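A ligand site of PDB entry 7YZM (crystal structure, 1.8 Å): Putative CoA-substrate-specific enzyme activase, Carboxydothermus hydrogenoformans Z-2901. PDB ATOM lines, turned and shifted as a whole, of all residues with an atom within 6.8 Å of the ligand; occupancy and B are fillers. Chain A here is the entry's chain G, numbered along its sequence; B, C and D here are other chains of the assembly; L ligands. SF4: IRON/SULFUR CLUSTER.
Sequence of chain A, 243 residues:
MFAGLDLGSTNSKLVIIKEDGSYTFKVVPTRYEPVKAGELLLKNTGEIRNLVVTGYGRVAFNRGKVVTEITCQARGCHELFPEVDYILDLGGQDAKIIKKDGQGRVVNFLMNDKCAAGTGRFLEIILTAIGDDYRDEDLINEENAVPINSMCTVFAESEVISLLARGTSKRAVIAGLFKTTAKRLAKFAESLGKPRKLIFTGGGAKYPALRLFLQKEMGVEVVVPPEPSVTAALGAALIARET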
ATOM      1  N   LYS A 114      32.329 -20.041  30.757  1.00  0.00           N
ATOM      2  CA  LYS A 114      31.786 -21.132  31.560  1.00  0.00           C
ATOM      3  C   LYS A 114      32.100 -22.493  30.958  1.00  0.00           C
ATOM      4  O   LYS A 114      32.370 -23.466  31.673  1.00  0.00           O
ATOM      5  CB  LYS A 114      30.268 -20.972  31.701  1.00  0.00           C
ATOM      6  CG  LYS A 114      29.797 -20.361  33.005  1.00  0.00           C
ATOM      7  CD  LYS A 114      28.309 -20.026  32.958  1.00  0.00           C
ATOM      8  CE  LYS A 114      27.466 -21.138  33.568  1.00  0.00           C
ATOM      9  NZ  LYS A 114      27.511 -21.096  35.055  1.00  0.00           N
ATOM     10  N   CYS A 115      32.023 -22.604  29.626  1.00  0.00           N
ATOM     11  CA  CYS A 115      32.260 -23.864  28.948  1.00  0.00           C
ATOM     12  C   CYS A 115      33.726 -24.267  28.953  1.00  0.00           C
ATOM     13  O   CYS A 115      34.040 -25.437  28.656  1.00  0.00           O
ATOM     14  CB  CYS A 115      31.752 -23.796  27.507  1.00  0.00           C
ATOM     15  SG  CYS A 115      29.964 -23.656  27.416  1.00  0.00           S
ATOM     16  N   ALA A 116      34.631 -23.346  29.264  1.00  0.00           N
ATOM     17  CA  ALA A 116      36.067 -23.623  29.316  1.00  0.00           C
ATOM     18  C   ALA A 116      36.570 -23.940  30.714  1.00  0.00           C
ATOM     19  O   ALA A 116      37.775 -24.055  30.925  1.00  0.00           O
ATOM     20  CB  ALA A 116      36.835 -22.430  28.731  1.00  0.00           C
ATOM     21  N   ALA A 117      35.672 -24.087  31.685  1.00  0.00           N
ATOM     22  CA  ALA A 117      36.073 -24.379  33.049  1.00  0.00           C
ATOM     23  C   ALA A 117      36.618 -25.795  33.181  1.00  0.00           C
ATOM     24  O   ALA A 117      36.177 -26.721  32.491  1.00  0.00           O
ATOM     25  CB  ALA A 117      34.895 -24.197  34.006  1.00  0.00           C
ATOM     26  N   MET A 151      36.006 -27.642  22.521  1.00  0.00           N
ATOM     27  CA  MET A 151      34.850 -26.960  23.113  1.00  0.00           C
ATOM     28  C   MET A 151      34.911 -26.954  24.634  1.00  0.00           C
ATOM     29  O   MET A 151      34.760 -25.906  25.267  1.00  0.00           O
ATOM     30  CB  MET A 151      33.553 -27.635  22.627  1.00  0.00           C
ATOM     31  CG  MET A 151      32.282 -26.956  23.136  1.00  0.00           C
ATOM     32  SD  MET A 151      31.906 -25.406  22.285  1.00  0.00           S
ATOM     33  CE  MET A 151      31.645 -24.309  23.668  1.00  0.00           C
ATOM     34  N   CYS A 152      35.108 -28.119  25.243  1.00  0.00           N
ATOM     35  CA  CYS A 152      34.980 -28.273  26.685  1.00  0.00           C
ATOM     36  C   CYS A 152      35.472 -29.661  27.043  1.00  0.00           C
ATOM     37  O   CYS A 152      35.715 -30.498  26.170  1.00  0.00           O
ATOM     38  CB  CYS A 152      33.544 -28.069  27.152  1.00  0.00           C
ATOM     39  SG  CYS A 152      32.523 -29.397  26.498  1.00  0.00           S
ATOM     40  N   THR A 153      35.591 -29.918  28.346  1.00  0.00           N
ATOM     41  CA  THR A 153      36.098 -31.212  28.799  1.00  0.00           C
ATOM     42  C   THR A 153      35.073 -32.329  28.601  1.00  0.00           C
ATOM     43  O   THR A 153      35.467 -33.485  28.496  1.00  0.00           O
ATOM     44  CB  THR A 153      36.525 -31.133  30.257  1.00  0.00           C
ATOM     45  OG1 THR A 153      35.425 -30.728  31.078  1.00  0.00           O
ATOM     46  CG2 THR A 153      37.663 -30.129  30.422  1.00  0.00           C
ATOM     47  N   VAL A 154      33.778 -32.008  28.570  1.00  0.00           N
ATOM     48  CA  VAL A 154      32.786 -33.032  28.270  1.00  0.00           C
ATOM     49  C   VAL A 154      33.002 -33.579  26.861  1.00  0.00           C
ATOM     50  O   VAL A 154      33.093 -34.797  26.660  1.00  0.00           O
ATOM     51  CB  VAL A 154      31.357 -32.474  28.446  1.00  0.00           C
ATOM     52  CG1 VAL A 154      30.323 -33.450  27.898  1.00  0.00           C
ATOM     53  CG2 VAL A 154      31.093 -32.158  29.911  1.00  0.00           C
ATOM     54  N   PHE A 155      33.082 -32.682  25.875  1.00  0.00           N
ATOM     55  CA  PHE A 155      33.268 -33.127  24.496  1.00  0.00           C
ATOM     56  C   PHE A 155      34.615 -33.825  24.333  1.00  0.00           C
ATOM     57  O   PHE A 155      34.714 -34.842  23.638  1.00  0.00           O
ATOM     58  CB  PHE A 155      33.156 -31.939  23.531  1.00  0.00           C
ATOM     59  CG  PHE A 155      31.773 -31.342  23.434  1.00  0.00           C
ATOM     60  CD1 PHE A 155      30.794 -31.615  24.378  1.00  0.00           C
ATOM     61  CD2 PHE A 155      31.452 -30.480  22.384  1.00  0.00           C
ATOM     62  CE1 PHE A 155      29.531 -31.055  24.279  1.00  0.00           C
ATOM     63  CE2 PHE A 155      30.189 -29.919  22.285  1.00  0.00           C
ATOM     64  CZ  PHE A 155      29.236 -30.211  23.239  1.00  0.00           C
ATOM     65  N   LYS B 114      24.973 -34.373  23.515  1.00  0.00           N
ATOM     66  CA  LYS B 114      26.410 -34.221  23.717  1.00  0.00           C
ATOM     67  C   LYS B 114      26.725 -33.576  25.056  1.00  0.00           C
ATOM     68  O   LYS B 114      27.664 -33.989  25.749  1.00  0.00           O
ATOM     69  CB  LYS B 114      27.031 -33.405  22.569  1.00  0.00           C
ATOM     70  CG  LYS B 114      27.387 -34.216  21.315  1.00  0.00           C
ATOM     71  CD  LYS B 114      28.025 -33.343  20.225  1.00  0.00           C
ATOM     72  CE  LYS B 114      29.544 -33.177  20.405  1.00  0.00           C
ATOM     73  NZ  LYS B 114      30.231 -34.279  21.157  1.00  0.00           N
ATOM     74  N   CYS B 115      25.965 -32.538  25.434  1.00  0.00           N
ATOM     75  CA  CYS B 115      26.253 -31.837  26.674  1.00  0.00           C
ATOM     76  C   CYS B 115      25.934 -32.674  27.899  1.00  0.00           C
ATOM     77  O   CYS B 115      26.357 -32.322  29.008  1.00  0.00           O
ATOM     78  CB  CYS B 115      25.467 -30.537  26.737  1.00  0.00           C
ATOM     79  SG  CYS B 115      25.975 -29.309  25.519  1.00  0.00           S
ATOM     80  N   ALA B 116      25.189 -33.770  27.735  1.00  0.00           N
ATOM     81  CA  ALA B 116      24.811 -34.627  28.848  1.00  0.00           C
ATOM     82  C   ALA B 116      25.721 -35.835  28.983  1.00  0.00           C
ATOM     83  O   ALA B 116      25.416 -36.741  29.775  1.00  0.00           O
ATOM     84  CB  ALA B 116      23.351 -35.070  28.682  1.00  0.00           C
ATOM     85  N   ALA B 117      26.818 -35.880  28.238  1.00  0.00           N
ATOM     86  CA  ALA B 117      27.736 -37.001  28.283  1.00  0.00           C
ATOM     87  C   ALA B 117      28.505 -37.026  29.601  1.00  0.00           C
ATOM     88  O   ALA B 117      28.790 -35.990  30.204  1.00  0.00           O
ATOM     89  CB  ALA B 117      28.722 -36.938  27.113  1.00  0.00           C
ATOM     90  N   MET B 151      22.966 -28.725  33.679  1.00  0.00           N
ATOM     91  CA  MET B 151      23.382 -28.595  32.283  1.00  0.00           C
ATOM     92  C   MET B 151      24.343 -29.706  31.883  1.00  0.00           C
ATOM     93  O   MET B 151      24.120 -30.429  30.906  1.00  0.00           O
ATOM     94  CB  MET B 151      24.028 -27.240  32.051  1.00  0.00           C
ATOM     95  CG  MET B 151      24.422 -27.017  30.607  1.00  0.00           C
ATOM     96  SD  MET B 151      22.970 -26.286  29.816  1.00  0.00           S
ATOM     97  CE  MET B 151      22.894 -27.179  28.301  1.00  0.00           C
ATOM     98  N   CYS B 152      25.443 -29.834  32.615  1.00  0.00           N
ATOM     99  CA  CYS B 152      26.532 -30.717  32.215  1.00  0.00           C
ATOM    100  C   CYS B 152      27.485 -30.853  33.389  1.00  0.00           C
ATOM    101  O   CYS B 152      27.357 -30.160  34.401  1.00  0.00           O
ATOM    102  CB  CYS B 152      27.270 -30.163  30.987  1.00  0.00           C
ATOM    103  SG  CYS B 152      28.073 -28.588  31.406  1.00  0.00           S
ATOM    104  N   THR B 153      28.454 -31.756  33.234  1.00  0.00           N
ATOM    105  CA  THR B 153      29.411 -32.014  34.303  1.00  0.00           C
ATOM    106  C   THR B 153      30.413 -30.881  34.478  1.00  0.00           C
ATOM    107  O   THR B 153      30.971 -30.733  35.564  1.00  0.00           O
ATOM    108  CB  THR B 153      30.145 -33.324  34.024  1.00  0.00           C
ATOM    109  OG1 THR B 153      30.842 -33.219  32.783  1.00  0.00           O
ATOM    110  CG2 THR B 153      29.154 -34.479  33.953  1.00  0.00           C
ATOM    111  N   VAL B 154      30.637 -30.071  33.438  1.00  0.00           N
ATOM    112  CA  VAL B 154      31.503 -28.909  33.592  1.00  0.00           C
ATOM    113  C   VAL B 154      30.883 -27.902  34.546  1.00  0.00           C
ATOM    114  O   VAL B 154      31.510 -27.453  35.508  1.00  0.00           O
ATOM    115  CB  VAL B 154      31.790 -28.265  32.225  1.00  0.00           C
ATOM    116  CG1 VAL B 154      32.465 -26.897  32.417  1.00  0.00           C
ATOM    117  CG2 VAL B 154      32.662 -29.172  31.384  1.00  0.00           C
ATOM    118  N   PHE B 155      29.638 -27.495  34.263  1.00  0.00           N
ATOM    119  CA  PHE B 155      28.990 -26.500  35.111  1.00  0.00           C
ATOM    120  C   PHE B 155      28.787 -27.048  36.511  1.00  0.00           C
ATOM    121  O   PHE B 155      28.887 -26.302  37.494  1.00  0.00           O
ATOM    122  CB  PHE B 155      27.635 -26.089  34.521  1.00  0.00           C
ATOM    123  CG  PHE B 155      27.702 -25.336  33.231  1.00  0.00           C
ATOM    124  CD1 PHE B 155      28.873 -25.274  32.486  1.00  0.00           C
ATOM    125  CD2 PHE B 155      26.578 -24.700  32.731  1.00  0.00           C
ATOM    126  CE1 PHE B 155      28.912 -24.603  31.282  1.00  0.00           C
ATOM    127  CE2 PHE B 155      26.618 -24.012  31.538  1.00  0.00           C
ATOM    128  CZ  PHE B 155      27.791 -23.962  30.811  1.00  0.00           C
ATOM    129  N   ARG C 111      18.274 -28.257  25.412  1.00  0.00           N
ATOM    130  CA  ARG C 111      18.937 -27.843  26.655  1.00  0.00           C
ATOM    131  C   ARG C 111      19.904 -26.683  26.416  1.00  0.00           C
ATOM    132  O   ARG C 111      20.136 -25.883  27.334  1.00  0.00           O
ATOM    133  CB  ARG C 111      19.612 -29.058  27.289  1.00  0.00           C
ATOM    134  CG  ARG C 111      18.603 -30.184  27.674  1.00  0.00           C
ATOM    135  CD  ARG C 111      19.191 -31.316  28.545  1.00  0.00           C
ATOM    136  NE  ARG C 111      20.581 -31.590  28.164  1.00  0.00           N
ATOM    137  CZ  ARG C 111      21.617 -31.404  28.968  1.00  0.00           C
ATOM    138  NH1 ARG C 111      22.839 -31.647  28.530  1.00  0.00           N
ATOM    139  NH2 ARG C 111      21.439 -30.989  30.215  1.00  0.00           N
ATOM    140  N   ASN C 112      20.444 -26.544  25.200  1.00  0.00           N
ATOM    141  CA  ASN C 112      21.307 -25.407  24.855  1.00  0.00           C
ATOM    142  C   ASN C 112      20.470 -24.230  24.335  1.00  0.00           C
ATOM    143  O   ASN C 112      20.649 -23.754  23.219  1.00  0.00           O
ATOM    144  CB  ASN C 112      22.334 -25.797  23.801  1.00  0.00           C
ATOM    145  CG  ASN C 112      23.352 -26.778  24.295  1.00  0.00           C
ATOM    146  OD1 ASN C 112      23.727 -26.765  25.460  1.00  0.00           O
ATOM    147  ND2 ASN C 112      23.832 -27.625  23.393  1.00  0.00           N
ATOM    148  N   GLN C 372      23.304 -17.275  29.278  1.00  0.00           N
ATOM    149  CA  GLN C 372      23.866 -18.340  28.464  1.00  0.00           C
ATOM    150  C   GLN C 372      22.940 -18.700  27.308  1.00  0.00           C
ATOM    151  O   GLN C 372      21.724 -18.825  27.488  1.00  0.00           O
ATOM    152  CB  GLN C 372      24.150 -19.561  29.348  1.00  0.00           C
ATOM    153  CG  GLN C 372      24.996 -20.637  28.687  1.00  0.00           C
ATOM    154  CD  GLN C 372      26.473 -20.512  29.000  1.00  0.00           C
ATOM    155  OE1 GLN C 372      26.913 -19.569  29.664  1.00  0.00           O
ATOM    156  NE2 GLN C 372      27.253 -21.469  28.520  1.00  0.00           N
ATOM    157  N   PHE C 373      23.535 -18.843  26.114  1.00  0.00           N
ATOM    158  CA  PHE C 373      22.882 -19.217  24.864  1.00  0.00           C
ATOM    159  C   PHE C 373      21.971 -18.130  24.318  1.00  0.00           C
ATOM    160  O   PHE C 373      21.197 -18.378  23.384  1.00  0.00           O
ATOM    161  CB  PHE C 373      22.108 -20.542  25.003  1.00  0.00           C
ATOM    162  CG  PHE C 373      22.920 -21.633  25.647  1.00  0.00           C
ATOM    163  CD1 PHE C 373      24.067 -22.126  25.026  1.00  0.00           C
ATOM    164  CD2 PHE C 373      22.556 -22.157  26.874  1.00  0.00           C
ATOM    165  CE1 PHE C 373      24.825 -23.116  25.628  1.00  0.00           C
ATOM    166  CE2 PHE C 373      23.313 -23.147  27.477  1.00  0.00           C
ATOM    167  CZ  PHE C 373      24.454 -23.624  26.851  1.00  0.00           C
ATOM    168  N   ARG D 111      31.789 -18.923  21.495  1.00  0.00           N
ATOM    169  CA  ARG D 111      32.087 -20.330  21.247  1.00  0.00           C
ATOM    170  C   ARG D 111      30.803 -21.152  21.173  1.00  0.00           C
ATOM    171  O   ARG D 111      30.750 -22.148  20.433  1.00  0.00           O
ATOM    172  CB  ARG D 111      33.041 -20.868  22.318  1.00  0.00           C
ATOM    173  CG  ARG D 111      34.344 -20.049  22.397  1.00  0.00           C
ATOM    174  CD  ARG D 111      35.494 -20.801  23.083  1.00  0.00           C
ATOM    175  NE  ARG D 111      35.057 -21.375  24.351  1.00  0.00           N
ATOM    176  CZ  ARG D 111      35.297 -22.626  24.729  1.00  0.00           C
ATOM    177  NH1 ARG D 111      34.840 -23.066  25.889  1.00  0.00           N
ATOM    178  NH2 ARG D 111      36.003 -23.439  23.950  1.00  0.00           N
ATOM    179  N   ASN D 112      29.758 -20.747  21.902  1.00  0.00           N
ATOM    180  CA  ASN D 112      28.447 -21.386  21.827  1.00  0.00           C
ATOM    181  C   ASN D 112      27.620 -20.874  20.648  1.00  0.00           C
ATOM    182  O   ASN D 112      26.497 -20.402  20.835  1.00  0.00           O
ATOM    183  CB  ASN D 112      27.607 -21.131  23.077  1.00  0.00           C
ATOM    184  CG  ASN D 112      28.178 -21.758  24.306  1.00  0.00           C
ATOM    185  OD1 ASN D 112      28.798 -22.818  24.251  1.00  0.00           O
ATOM    186  ND2 ASN D 112      27.952 -21.120  25.457  1.00  0.00           N
ATOM    187  N   GLN D 372      25.227 -28.390  16.182  1.00  0.00           N
ATOM    188  CA  GLN D 372      25.209 -27.896  17.557  1.00  0.00           C
ATOM    189  C   GLN D 372      25.016 -26.386  17.598  1.00  0.00           C
ATOM    190  O   GLN D 372      25.656 -25.639  16.854  1.00  0.00           O
ATOM    191  CB  GLN D 372      26.522 -28.304  18.233  1.00  0.00           C
ATOM    192  CG  GLN D 372      26.593 -28.104  19.736  1.00  0.00           C
ATOM    193  CD  GLN D 372      26.085 -29.300  20.532  1.00  0.00           C
ATOM    194  OE1 GLN D 372      26.039 -30.426  20.037  1.00  0.00           O
ATOM    195  NE2 GLN D 372      25.709 -29.039  21.778  1.00  0.00           N
ATOM    196  N   PHE D 373      24.100 -25.951  18.460  1.00  0.00           N
ATOM    197  CA  PHE D 373      23.758 -24.547  18.714  1.00  0.00           C
ATOM    198  C   PHE D 373      22.952 -23.914  17.587  1.00  0.00           C
ATOM    199  O   PHE D 373      22.737 -22.704  17.608  1.00  0.00           O
ATOM    200  CB  PHE D 373      25.020 -23.713  19.002  1.00  0.00           C
ATOM    201  CG  PHE D 373      25.846 -24.281  20.104  1.00  0.00           C
ATOM    202  CD1 PHE D 373      25.352 -24.343  21.402  1.00  0.00           C
ATOM    203  CD2 PHE D 373      27.114 -24.773  19.871  1.00  0.00           C
ATOM    204  CE1 PHE D 373      26.101 -24.878  22.421  1.00  0.00           C
ATOM    205  CE2 PHE D 373      27.872 -25.318  20.886  1.00  0.00           C
ATOM    206  CZ  PHE D 373      27.365 -25.374  22.158  1.00  0.00           C
HETATM  207 FE1  SF4 L   1      28.671 -27.946  29.197  1.00  0.00          FE
HETATM  208 FE2  SF4 L   1      27.760 -28.125  26.650  1.00  0.00          FE
HETATM  209 FE3  SF4 L   1      30.401 -28.378  27.134  1.00  0.00          FE
HETATM  210 FE4  SF4 L   1      29.218 -25.961  27.414  1.00  0.00          FE
HETATM  211  S1  SF4 L   1      29.443 -27.149  25.489  1.00  0.00           S
HETATM  212  S2  SF4 L   1      30.683 -26.928  28.874  1.00  0.00           S
HETATM  213  S3  SF4 L   1      27.172 -26.557  28.184  1.00  0.00           S
HETATM  214  S4  SF4 L   1      28.752 -29.785  27.879  1.00  0.00           S
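SG of Cys 152 of chain B binds FE1 of the ligand (2.4 Å).
An iron atom (FE2) of the ligand is bound by the side-chain sulfur (SG) of Cys 115 of chain B, 2.4 Å away.
The side-chain sulfur (SG) of Cys 115 of chain A binds an iron atom (FE4) of the ligand, at 2.4 Å.
The side-chain sulfur (SG) of Cys 152 of chain A binds an iron atom (FE3) of the ligand (2.4 Å).
SG of Cys 115 of chain B lies close to NE2 of Gln 372 of chain D (3.8 Å).
NH2 of Arg 111 of chain C lies within hydrogen-bond range of O of Met 151 of chain B (2.8 Å).
The side-chain sulfur (SG) of Cys 115 of chain A lies close to the side-chain amide oxygen (OD1) of Asn 112 of chain D, 3.5 Å away.
SG of Cys 152 of chain B sits close to N of Phe 155 of chain B (3.4 Å).
The backbone carbonyl oxygen (O) of Met 151 of chain A sits at hydrogen-bond distance from the guanidinium group (NH1) of Arg 111 of chain D, at 2.9 Å.
The side-chain sulfur (SG) of Cys 152 of chain A sits close to the backbone NH (N) of Phe 155 of chain A.
The side-chain sulfur of Cys 152 of chain A lies close to the backbone NH of Val 154 of chain A.
The side-chain sulfur (SG) of Cys 152 of chain B sits close to the backbone NH (N) of Val 154 of chain B (3.6 Å).
Merely in contact with the ligand: Met 151 of chain A (3.7 Å), Val 154 of chain A (3.8 Å), Phe 155 of chain A (3.8 Å), Met 151 of chain B (3.7 Å), Val 154 of chain B (3.8 Å) and Phe 155 of chain B (3.7 Å).
Hydrophobic or aromatic side chains within 4 Å of the ligand: Met 151 of chain A, Val 154 of chain A, Phe 155 of chain A, Met 151 of chain B, Val 154 of chain B and Phe 155 of chain B.
Within 4 Å of the ligand: Cys 115 of chain A, Met 151 of chain A, Cys 152 of chain A, Val 154 of chain A, Phe 155 of chain A, Cys 115 of chain B, Met 151 of chain B, Cys 152 of chain B, Val 154 of chain B and Phe 155 of chain B.
The nearest printed residue that does not touch the ligand is Phe 373 of chain C (4.2 Å).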
